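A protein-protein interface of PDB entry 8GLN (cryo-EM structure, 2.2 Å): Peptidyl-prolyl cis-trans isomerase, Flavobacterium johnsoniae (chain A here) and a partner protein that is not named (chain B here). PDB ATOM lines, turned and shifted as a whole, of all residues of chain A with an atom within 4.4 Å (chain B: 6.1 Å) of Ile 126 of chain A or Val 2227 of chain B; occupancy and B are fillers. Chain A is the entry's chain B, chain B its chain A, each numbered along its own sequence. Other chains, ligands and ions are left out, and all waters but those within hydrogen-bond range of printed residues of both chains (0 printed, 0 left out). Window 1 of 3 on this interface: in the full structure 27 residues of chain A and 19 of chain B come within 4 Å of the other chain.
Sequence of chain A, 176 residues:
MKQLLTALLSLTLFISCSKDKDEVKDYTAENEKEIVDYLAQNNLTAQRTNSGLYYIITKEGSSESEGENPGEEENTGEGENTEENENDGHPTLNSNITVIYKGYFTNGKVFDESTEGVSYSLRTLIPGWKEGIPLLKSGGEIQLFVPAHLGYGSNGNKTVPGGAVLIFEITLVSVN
N of Val 2227 of chain B lies within hydrogen-bond range of O of Thr 124 of chain A.
The backbone carbonyl oxygen (O) of Pro 2225 of chain B is in hydrogen-bond range of the backbone NH (N) of Ile 126 of chain A, 3.1 Å away.
O of Ser 2224 of chain B sits at hydrogen-bond distance from OH of Tyr 152 of chain A.
NZ of Lys 2226 of chain B is in hydrogen-bond range of OG1 of Thr 124 of chain A.
The backbone NH (N) of Gln 2228 of chain B sits at hydrogen-bond distance from the backbone carbonyl oxygen (O) of Thr 124 of chain A.
The side-chain amide oxygen of Gln 2228 of chain B is in hydrogen-bond range of the side-chain amino group of Lys 130 of chain A.
NZ of Lys 2226 of chain B sits at hydrogen-bond distance from O of Gln 2228 of chain B (3.2 Å).
The backbone carbonyl oxygen (O) of Val 2227 of chain B sits at hydrogen-bond distance from the backbone NH (N) of Tyr 2235 of chain B (3.1 Å).
OD1 of Asn 2222 of chain B lies within hydrogen-bond range of OG of Ser 2224 of chain B (2.4 Å).
NZ of Lys 2226 of chain B sits close to OH of Tyr 2235 of chain B (3.2 Å).
Of the 11 printed residues of chain A, 6 touch a printed residue of chain B.
Hydrophobic or aromatic side chains of chain A that line the printed part of chain B: Leu 125, Ile 126, Trp 129 and Tyr 152.
Of the 10 printed residues of chain B, 5 touch a printed residue of chain A.
Hydrophobic or aromatic side chains of chain B within 4 Å of the printed part of chain A: Pro 2225 and Val 2227.
Among the printed residues, no Asp or Glu carboxylate lies within 4 Å of a Lys or Arg side-chain nitrogen of the other chain.
Printed residues of chain A within 4 Å of Val 2227 of chain B: Thr 124 (2.8 Å), Leu 125 (3.8 Å), Ile 126 (3.7 Å) and Tyr 152 (3.7 Å).
Printed residues of chain B within 4 Å of Thr 124 of chain A: Lys 2226 (3.3 Å), Val 2227 (2.8 Å) and Gln 2228 (2.9 Å).
Printed residues of chain A within 4 Å of Ser 2224 of chain B: Tyr 152 (3.1 Å).
Of the printed residues of chain B, Tyr 152 of chain A touches Ser 2224, Pro 2225 and Val 2227.
Printed residues of chain B within 4 Å of Lys 130 of chain A: Gln 2228.
Printed residues of chain A within 4 Å of Lys 2226 of chain B: Thr 124 (3.3 Å) and Leu 125 (3.7 Å).
The nearest residue of chain B that does not touch Ile 126 of chain A is Lys 2226 of chain B (5.2 Å).
The nearest printed residue of chain A that does not touch Val 2227 of chain B is Pro 127 of chain A (5.4 Å).
The nearest printed residue of chain B that does not touch Leu 125 of chain A is Gln 2228 of chain B (4.2 Å).
CA of Leu 125 of chain A touches O of Pro 2225 of chain B, 3.2 Å away.
Leu 125 of chain A touches Lys 2226 of chain B.
CG2 of Val 2227 of chain B touches C of Leu 125 of chain A, at 3.8 Å.
CG1 of Val 2227 of chain B touches CG2 of Ile 126 of chain A, at 3.7 Å.
Trp 129 of chain A touches Pro 2225 of chain B (CH2 to CG, 3.7 Å).
OH of Tyr 152 of chain A touches N of Pro 2225 of chain B, at 3.8 Å.
Val 2227 of chain B touches Tyr 152 of chain A (CG1 to CE1, 3.7 Å).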
ATOM      1  N   THR A 124      -2.701   0.574  22.859  1.00  0.00           N
ATOM      2  CA  THR A 124      -1.507   1.076  22.199  1.00  0.00           C
ATOM      3  C   THR A 124      -0.367   0.067  22.207  1.00  0.00           C
ATOM      4  O   THR A 124       0.724   0.380  21.722  1.00  0.00           O
ATOM      5  CB  THR A 124      -1.048   2.375  22.866  1.00  0.00           C
ATOM      6  OG1 THR A 124      -0.396   2.073  24.105  1.00  0.00           O
ATOM      7  CG2 THR A 124      -2.238   3.276  23.142  1.00  0.00           C
ATOM      8  N   LEU A 125      -0.591  -1.129  22.741  1.00  0.00           N
ATOM      9  CA  LEU A 125       0.446  -2.133  22.901  1.00  0.00           C
ATOM     10  C   LEU A 125       0.460  -3.084  21.706  1.00  0.00           C
ATOM     11  O   LEU A 125      -0.367  -2.999  20.795  1.00  0.00           O
ATOM     12  CB  LEU A 125       0.246  -2.897  24.212  1.00  0.00           C
ATOM     13  CG  LEU A 125      -0.075  -2.052  25.447  1.00  0.00           C
ATOM     14  CD1 LEU A 125      -0.323  -2.940  26.654  1.00  0.00           C
ATOM     15  CD2 LEU A 125       1.037  -1.058  25.733  1.00  0.00           C
ATOM     16  N   ILE A 126       1.421  -4.002  21.715  1.00  0.00           N
ATOM     17  CA  ILE A 126       1.568  -4.995  20.653  1.00  0.00           C
ATOM     18  C   ILE A 126       0.379  -5.949  20.699  1.00  0.00           C
ATOM     19  O   ILE A 126      -0.217  -6.140  21.769  1.00  0.00           O
ATOM     20  CB  ILE A 126       2.902  -5.749  20.778  1.00  0.00           C
ATOM     21  CG1 ILE A 126       3.065  -6.330  22.184  1.00  0.00           C
ATOM     22  CG2 ILE A 126       4.065  -4.833  20.443  1.00  0.00           C
ATOM     23  CD1 ILE A 126       4.236  -7.277  22.314  1.00  0.00           C
ATOM     24  N   PRO A 127      -0.007  -6.553  19.570  1.00  0.00           N
ATOM     25  CA  PRO A 127      -1.192  -7.427  19.572  1.00  0.00           C
ATOM     26  C   PRO A 127      -1.110  -8.580  20.555  1.00  0.00           C
ATOM     27  O   PRO A 127      -2.146  -8.995  21.092  1.00  0.00           O
ATOM     28  CB  PRO A 127      -1.250  -7.928  18.123  1.00  0.00           C
ATOM     29  CG  PRO A 127      -0.606  -6.848  17.335  1.00  0.00           C
ATOM     30  CD  PRO A 127       0.488  -6.298  18.206  1.00  0.00           C
ATOM     31  N   GLY A 128       0.087  -9.119  20.800  1.00  0.00           N
ATOM     32  CA  GLY A 128       0.213 -10.210  21.753  1.00  0.00           C
ATOM     33  C   GLY A 128      -0.304  -9.838  23.128  1.00  0.00           C
ATOM     34  O   GLY A 128      -1.023 -10.610  23.766  1.00  0.00           O
ATOM     35  N   TRP A 129       0.049  -8.642  23.598  1.00  0.00           N
ATOM     36  CA  TRP A 129      -0.501  -8.154  24.858  1.00  0.00           C
ATOM     37  C   TRP A 129      -2.006  -7.943  24.760  1.00  0.00           C
ATOM     38  O   TRP A 129      -2.744  -8.279  25.692  1.00  0.00           O
ATOM     39  CB  TRP A 129       0.197  -6.862  25.271  1.00  0.00           C
ATOM     40  CG  TRP A 129       1.566  -7.071  25.826  1.00  0.00           C
ATOM     41  CD1 TRP A 129       2.546  -7.870  25.316  1.00  0.00           C
ATOM     42  CD2 TRP A 129       2.112  -6.469  27.002  1.00  0.00           C
ATOM     43  NE1 TRP A 129       3.669  -7.802  26.103  1.00  0.00           N
ATOM     44  CE2 TRP A 129       3.427  -6.947  27.145  1.00  0.00           C
ATOM     45  CE3 TRP A 129       1.614  -5.569  27.949  1.00  0.00           C
ATOM     46  CZ2 TRP A 129       4.251  -6.557  28.196  1.00  0.00           C
ATOM     47  CZ3 TRP A 129       2.433  -5.183  28.989  1.00  0.00           C
ATOM     48  CH2 TRP A 129       3.734  -5.676  29.105  1.00  0.00           C
ATOM     49  N   LYS A 130      -2.479  -7.399  23.634  1.00  0.00           N
ATOM     50  CA  LYS A 130      -3.910  -7.170  23.462  1.00  0.00           C
ATOM     51  C   LYS A 130      -4.706  -8.464  23.565  1.00  0.00           C
ATOM     52  O   LYS A 130      -5.870  -8.443  23.976  1.00  0.00           O
ATOM     53  CB  LYS A 130      -4.180  -6.496  22.118  1.00  0.00           C
ATOM     54  CG  LYS A 130      -3.757  -5.043  22.041  1.00  0.00           C
ATOM     55  CD  LYS A 130      -4.087  -4.463  20.679  1.00  0.00           C
ATOM     56  CE  LYS A 130      -3.533  -3.061  20.522  1.00  0.00           C
ATOM     57  NZ  LYS A 130      -3.808  -2.505  19.170  1.00  0.00           N
ATOM     58  N   LEU A 150       2.821 -11.050  15.915  1.00  0.00           N
ATOM     59  CA  LEU A 150       2.071 -10.454  17.011  1.00  0.00           C
ATOM     60  C   LEU A 150       2.926  -9.534  17.871  1.00  0.00           C
ATOM     61  O   LEU A 150       2.407  -8.934  18.817  1.00  0.00           O
ATOM     62  CB  LEU A 150       1.449 -11.545  17.886  1.00  0.00           C
ATOM     63  CG  LEU A 150       0.280 -12.337  17.302  1.00  0.00           C
ATOM     64  CD1 LEU A 150      -0.452 -13.092  18.398  1.00  0.00           C
ATOM     65  CD2 LEU A 150      -0.672 -11.419  16.555  1.00  0.00           C
ATOM     66  N   GLY A 151       4.216  -9.411  17.570  1.00  0.00           N
ATOM     67  CA  GLY A 151       5.104  -8.576  18.354  1.00  0.00           C
ATOM     68  C   GLY A 151       5.571  -7.341  17.614  1.00  0.00           C
ATOM     69  O   GLY A 151       4.787  -6.417  17.382  1.00  0.00           O
ATOM     70  N   TYR A 152       6.847  -7.312  17.237  1.00  0.00           N
ATOM     71  CA  TYR A 152       7.428  -6.175  16.537  1.00  0.00           C
ATOM     72  C   TYR A 152       7.544  -6.403  15.035  1.00  0.00           C
ATOM     73  O   TYR A 152       8.135  -5.573  14.337  1.00  0.00           O
ATOM     74  CB  TYR A 152       8.795  -5.833  17.130  1.00  0.00           C
ATOM     75  CG  TYR A 152       8.722  -5.393  18.572  1.00  0.00           C
ATOM     76  CD1 TYR A 152       8.137  -4.183  18.917  1.00  0.00           C
ATOM     77  CD2 TYR A 152       9.232  -6.187  19.589  1.00  0.00           C
ATOM     78  CE1 TYR A 152       8.063  -3.775  20.234  1.00  0.00           C
ATOM     79  CE2 TYR A 152       9.163  -5.788  20.908  1.00  0.00           C
ATOM     80  CZ  TYR A 152       8.577  -4.580  21.225  1.00  0.00           C
ATOM     81  OH  TYR A 152       8.506  -4.177  22.537  1.00  0.00           O
ATOM     82  N   PHE A 168       7.303 -12.883  27.459  1.00  0.00           N
ATOM     83  CA  PHE A 168       6.902 -11.891  28.448  1.00  0.00           C
ATOM     84  C   PHE A 168       6.428 -12.589  29.714  1.00  0.00           C
ATOM     85  O   PHE A 168       5.689 -13.575  29.643  1.00  0.00           O
ATOM     86  CB  PHE A 168       5.792 -10.982  27.910  1.00  0.00           C
ATOM     87  CG  PHE A 168       6.273  -9.954  26.928  1.00  0.00           C
ATOM     88  CD1 PHE A 168       6.853  -8.778  27.368  1.00  0.00           C
ATOM     89  CD2 PHE A 168       6.137 -10.161  25.567  1.00  0.00           C
ATOM     90  CE1 PHE A 168       7.295  -7.830  26.469  1.00  0.00           C
ATOM     91  CE2 PHE A 168       6.577  -9.218  24.663  1.00  0.00           C
ATOM     92  CZ  PHE A 168       7.157  -8.050  25.114  1.00  0.00           C
ATOM     93  N   ASN B2222      10.841   3.038  21.102  1.00  0.00           N
ATOM     94  CA  ASN B2222      11.694   2.384  22.084  1.00  0.00           C
ATOM     95  C   ASN B2222      11.351   0.898  22.115  1.00  0.00           C
ATOM     96  O   ASN B2222      10.646   0.383  21.243  1.00  0.00           O
ATOM     97  CB  ASN B2222      11.541   3.059  23.454  1.00  0.00           C
ATOM     98  CG  ASN B2222      10.090   3.249  23.852  1.00  0.00           C
ATOM     99  OD1 ASN B2222       9.283   2.326  23.763  1.00  0.00           O
ATOM    100  ND2 ASN B2222       9.751   4.454  24.291  1.00  0.00           N
ATOM    101  N   SER B2224       9.687  -0.595  24.581  1.00  0.00           N
ATOM    102  CA  SER B2224       8.494  -0.861  25.364  1.00  0.00           C
ATOM    103  C   SER B2224       7.430  -1.529  24.493  1.00  0.00           C
ATOM    104  O   SER B2224       7.449  -1.398  23.266  1.00  0.00           O
ATOM    105  CB  SER B2224       7.955   0.439  25.957  1.00  0.00           C
ATOM    106  OG  SER B2224       7.418   1.273  24.947  1.00  0.00           O
ATOM    107  N   PRO B2225       6.489  -2.258  25.102  1.00  0.00           N
ATOM    108  CA  PRO B2225       5.407  -2.863  24.307  1.00  0.00           C
ATOM    109  C   PRO B2225       4.449  -1.848  23.707  1.00  0.00           C
ATOM    110  O   PRO B2225       3.663  -2.219  22.826  1.00  0.00           O
ATOM    111  CB  PRO B2225       4.692  -3.782  25.306  1.00  0.00           C
ATOM    112  CG  PRO B2225       5.089  -3.319  26.651  1.00  0.00           C
ATOM    113  CD  PRO B2225       6.317  -2.475  26.550  1.00  0.00           C
ATOM    114  N   LYS B2226       4.488  -0.593  24.147  1.00  0.00           N
ATOM    115  CA  LYS B2226       3.631   0.452  23.598  1.00  0.00           C
ATOM    116  C   LYS B2226       4.163   0.848  22.225  1.00  0.00           C
ATOM    117  O   LYS B2226       5.219   1.480  22.118  1.00  0.00           O
ATOM    118  CB  LYS B2226       3.587   1.643  24.553  1.00  0.00           C
ATOM    119  CG  LYS B2226       3.045   2.933  23.965  1.00  0.00           C
ATOM    120  CD  LYS B2226       2.766   3.938  25.072  1.00  0.00           C
ATOM    121  CE  LYS B2226       2.244   5.253  24.524  1.00  0.00           C
ATOM    122  NZ  LYS B2226       0.966   5.085  23.782  1.00  0.00           N
ATOM    123  N   VAL B2227       3.438   0.473  21.174  1.00  0.00           N
ATOM    124  CA  VAL B2227       3.892   0.690  19.804  1.00  0.00           C
ATOM    125  C   VAL B2227       2.977   1.605  19.005  1.00  0.00           C
ATOM    126  O   VAL B2227       3.375   2.051  17.920  1.00  0.00           O
ATOM    127  CB  VAL B2227       4.075  -0.647  19.054  1.00  0.00           C
ATOM    128  CG1 VAL B2227       5.273  -1.403  19.601  1.00  0.00           C
ATOM    129  CG2 VAL B2227       2.812  -1.487  19.157  1.00  0.00           C
ATOM    130  N   GLN B2228       1.777   1.904  19.488  1.00  0.00           N
ATOM    131  CA  GLN B2228       0.829   2.738  18.765  1.00  0.00           C
ATOM    132  C   GLN B2228       0.620   4.054  19.503  1.00  0.00           C
ATOM    133  O   GLN B2228       0.593   4.087  20.736  1.00  0.00           O
ATOM    134  CB  GLN B2228      -0.511   2.019  18.582  1.00  0.00           C
ATOM    135  CG  GLN B2228      -0.549   1.096  17.375  1.00  0.00           C
ATOM    136  CD  GLN B2228      -1.878   0.386  17.225  1.00  0.00           C
ATOM    137  OE1 GLN B2228      -2.171  -0.567  17.945  1.00  0.00           O
ATOM    138  NE2 GLN B2228      -2.691   0.845  16.282  1.00  0.00           N
ATOM    139  N   ASP B2229       0.480   5.135  18.743  1.00  0.00           N
ATOM    140  CA  ASP B2229       0.288   6.459  19.313  1.00  0.00           C
ATOM    141  C   ASP B2229      -1.203   6.728  19.525  1.00  0.00           C
ATOM    142  O   ASP B2229      -2.046   5.842  19.370  1.00  0.00           O
ATOM    143  CB  ASP B2229       0.975   7.511  18.437  1.00  0.00           C
ATOM    144  CG  ASP B2229       0.306   7.704  17.078  1.00  0.00           C
ATOM    145  OD1 ASP B2229      -0.732   7.076  16.792  1.00  0.00           O
ATOM    146  OD2 ASP B2229       0.841   8.500  16.279  1.00  0.00           O
ATOM    147  N   ASN B2233      -1.475   5.153  15.051  1.00  0.00           N
ATOM    148  CA  ASN B2233      -0.336   4.987  14.158  1.00  0.00           C
ATOM    149  C   ASN B2233       0.840   4.378  14.910  1.00  0.00           C
ATOM    150  O   ASN B2233       1.047   4.654  16.094  1.00  0.00           O
ATOM    151  CB  ASN B2233       0.080   6.330  13.554  1.00  0.00           C
ATOM    152  CG  ASN B2233      -0.908   6.841  12.527  1.00  0.00           C
ATOM    153  OD1 ASN B2233      -1.311   6.113  11.623  1.00  0.00           O
ATOM    154  ND2 ASN B2233      -1.294   8.103  12.655  1.00  0.00           N
ATOM    155  N   PHE B2234       1.610   3.542  14.217  1.00  0.00           N
ATOM    156  CA  PHE B2234       2.860   3.061  14.786  1.00  0.00           C
ATOM    157  C   PHE B2234       3.837   4.217  14.959  1.00  0.00           C
ATOM    158  O   PHE B2234       3.853   5.170  14.177  1.00  0.00           O
ATOM    159  CB  PHE B2234       3.487   1.984  13.900  1.00  0.00           C
ATOM    160  CG  PHE B2234       2.772   0.667  13.943  1.00  0.00           C
ATOM    161  CD1 PHE B2234       2.311   0.153  15.143  1.00  0.00           C
ATOM    162  CD2 PHE B2234       2.587  -0.074  12.788  1.00  0.00           C
ATOM    163  CE1 PHE B2234       1.657  -1.062  15.187  1.00  0.00           C
ATOM    164  CE2 PHE B2234       1.939  -1.293  12.826  1.00  0.00           C
ATOM    165  CZ  PHE B2234       1.471  -1.787  14.026  1.00  0.00           C
ATOM    166  N   TYR B2235       4.650   4.131  16.006  1.00  0.00           N
ATOM    167  CA  TYR B2235       5.663   5.149  16.243  1.00  0.00           C
ATOM    168  C   TYR B2235       6.751   5.079  15.180  1.00  0.00           C
ATOM    169  O   TYR B2235       7.155   3.996  14.748  1.00  0.00           O
ATOM    170  CB  TYR B2235       6.270   4.982  17.634  1.00  0.00           C
ATOM    171  CG  TYR B2235       5.348   5.426  18.740  1.00  0.00           C
ATOM    172  CD1 TYR B2235       4.984   6.759  18.866  1.00  0.00           C
ATOM    173  CD2 TYR B2235       4.836   4.518  19.655  1.00  0.00           C
ATOM    174  CE1 TYR B2235       4.141   7.176  19.871  1.00  0.00           C
ATOM    175  CE2 TYR B2235       3.990   4.926  20.665  1.00  0.00           C
ATOM    176  CZ  TYR B2235       3.646   6.257  20.767  1.00  0.00           C
ATOM    177  OH  TYR B2235       2.805   6.679  21.767  1.00  0.00           O
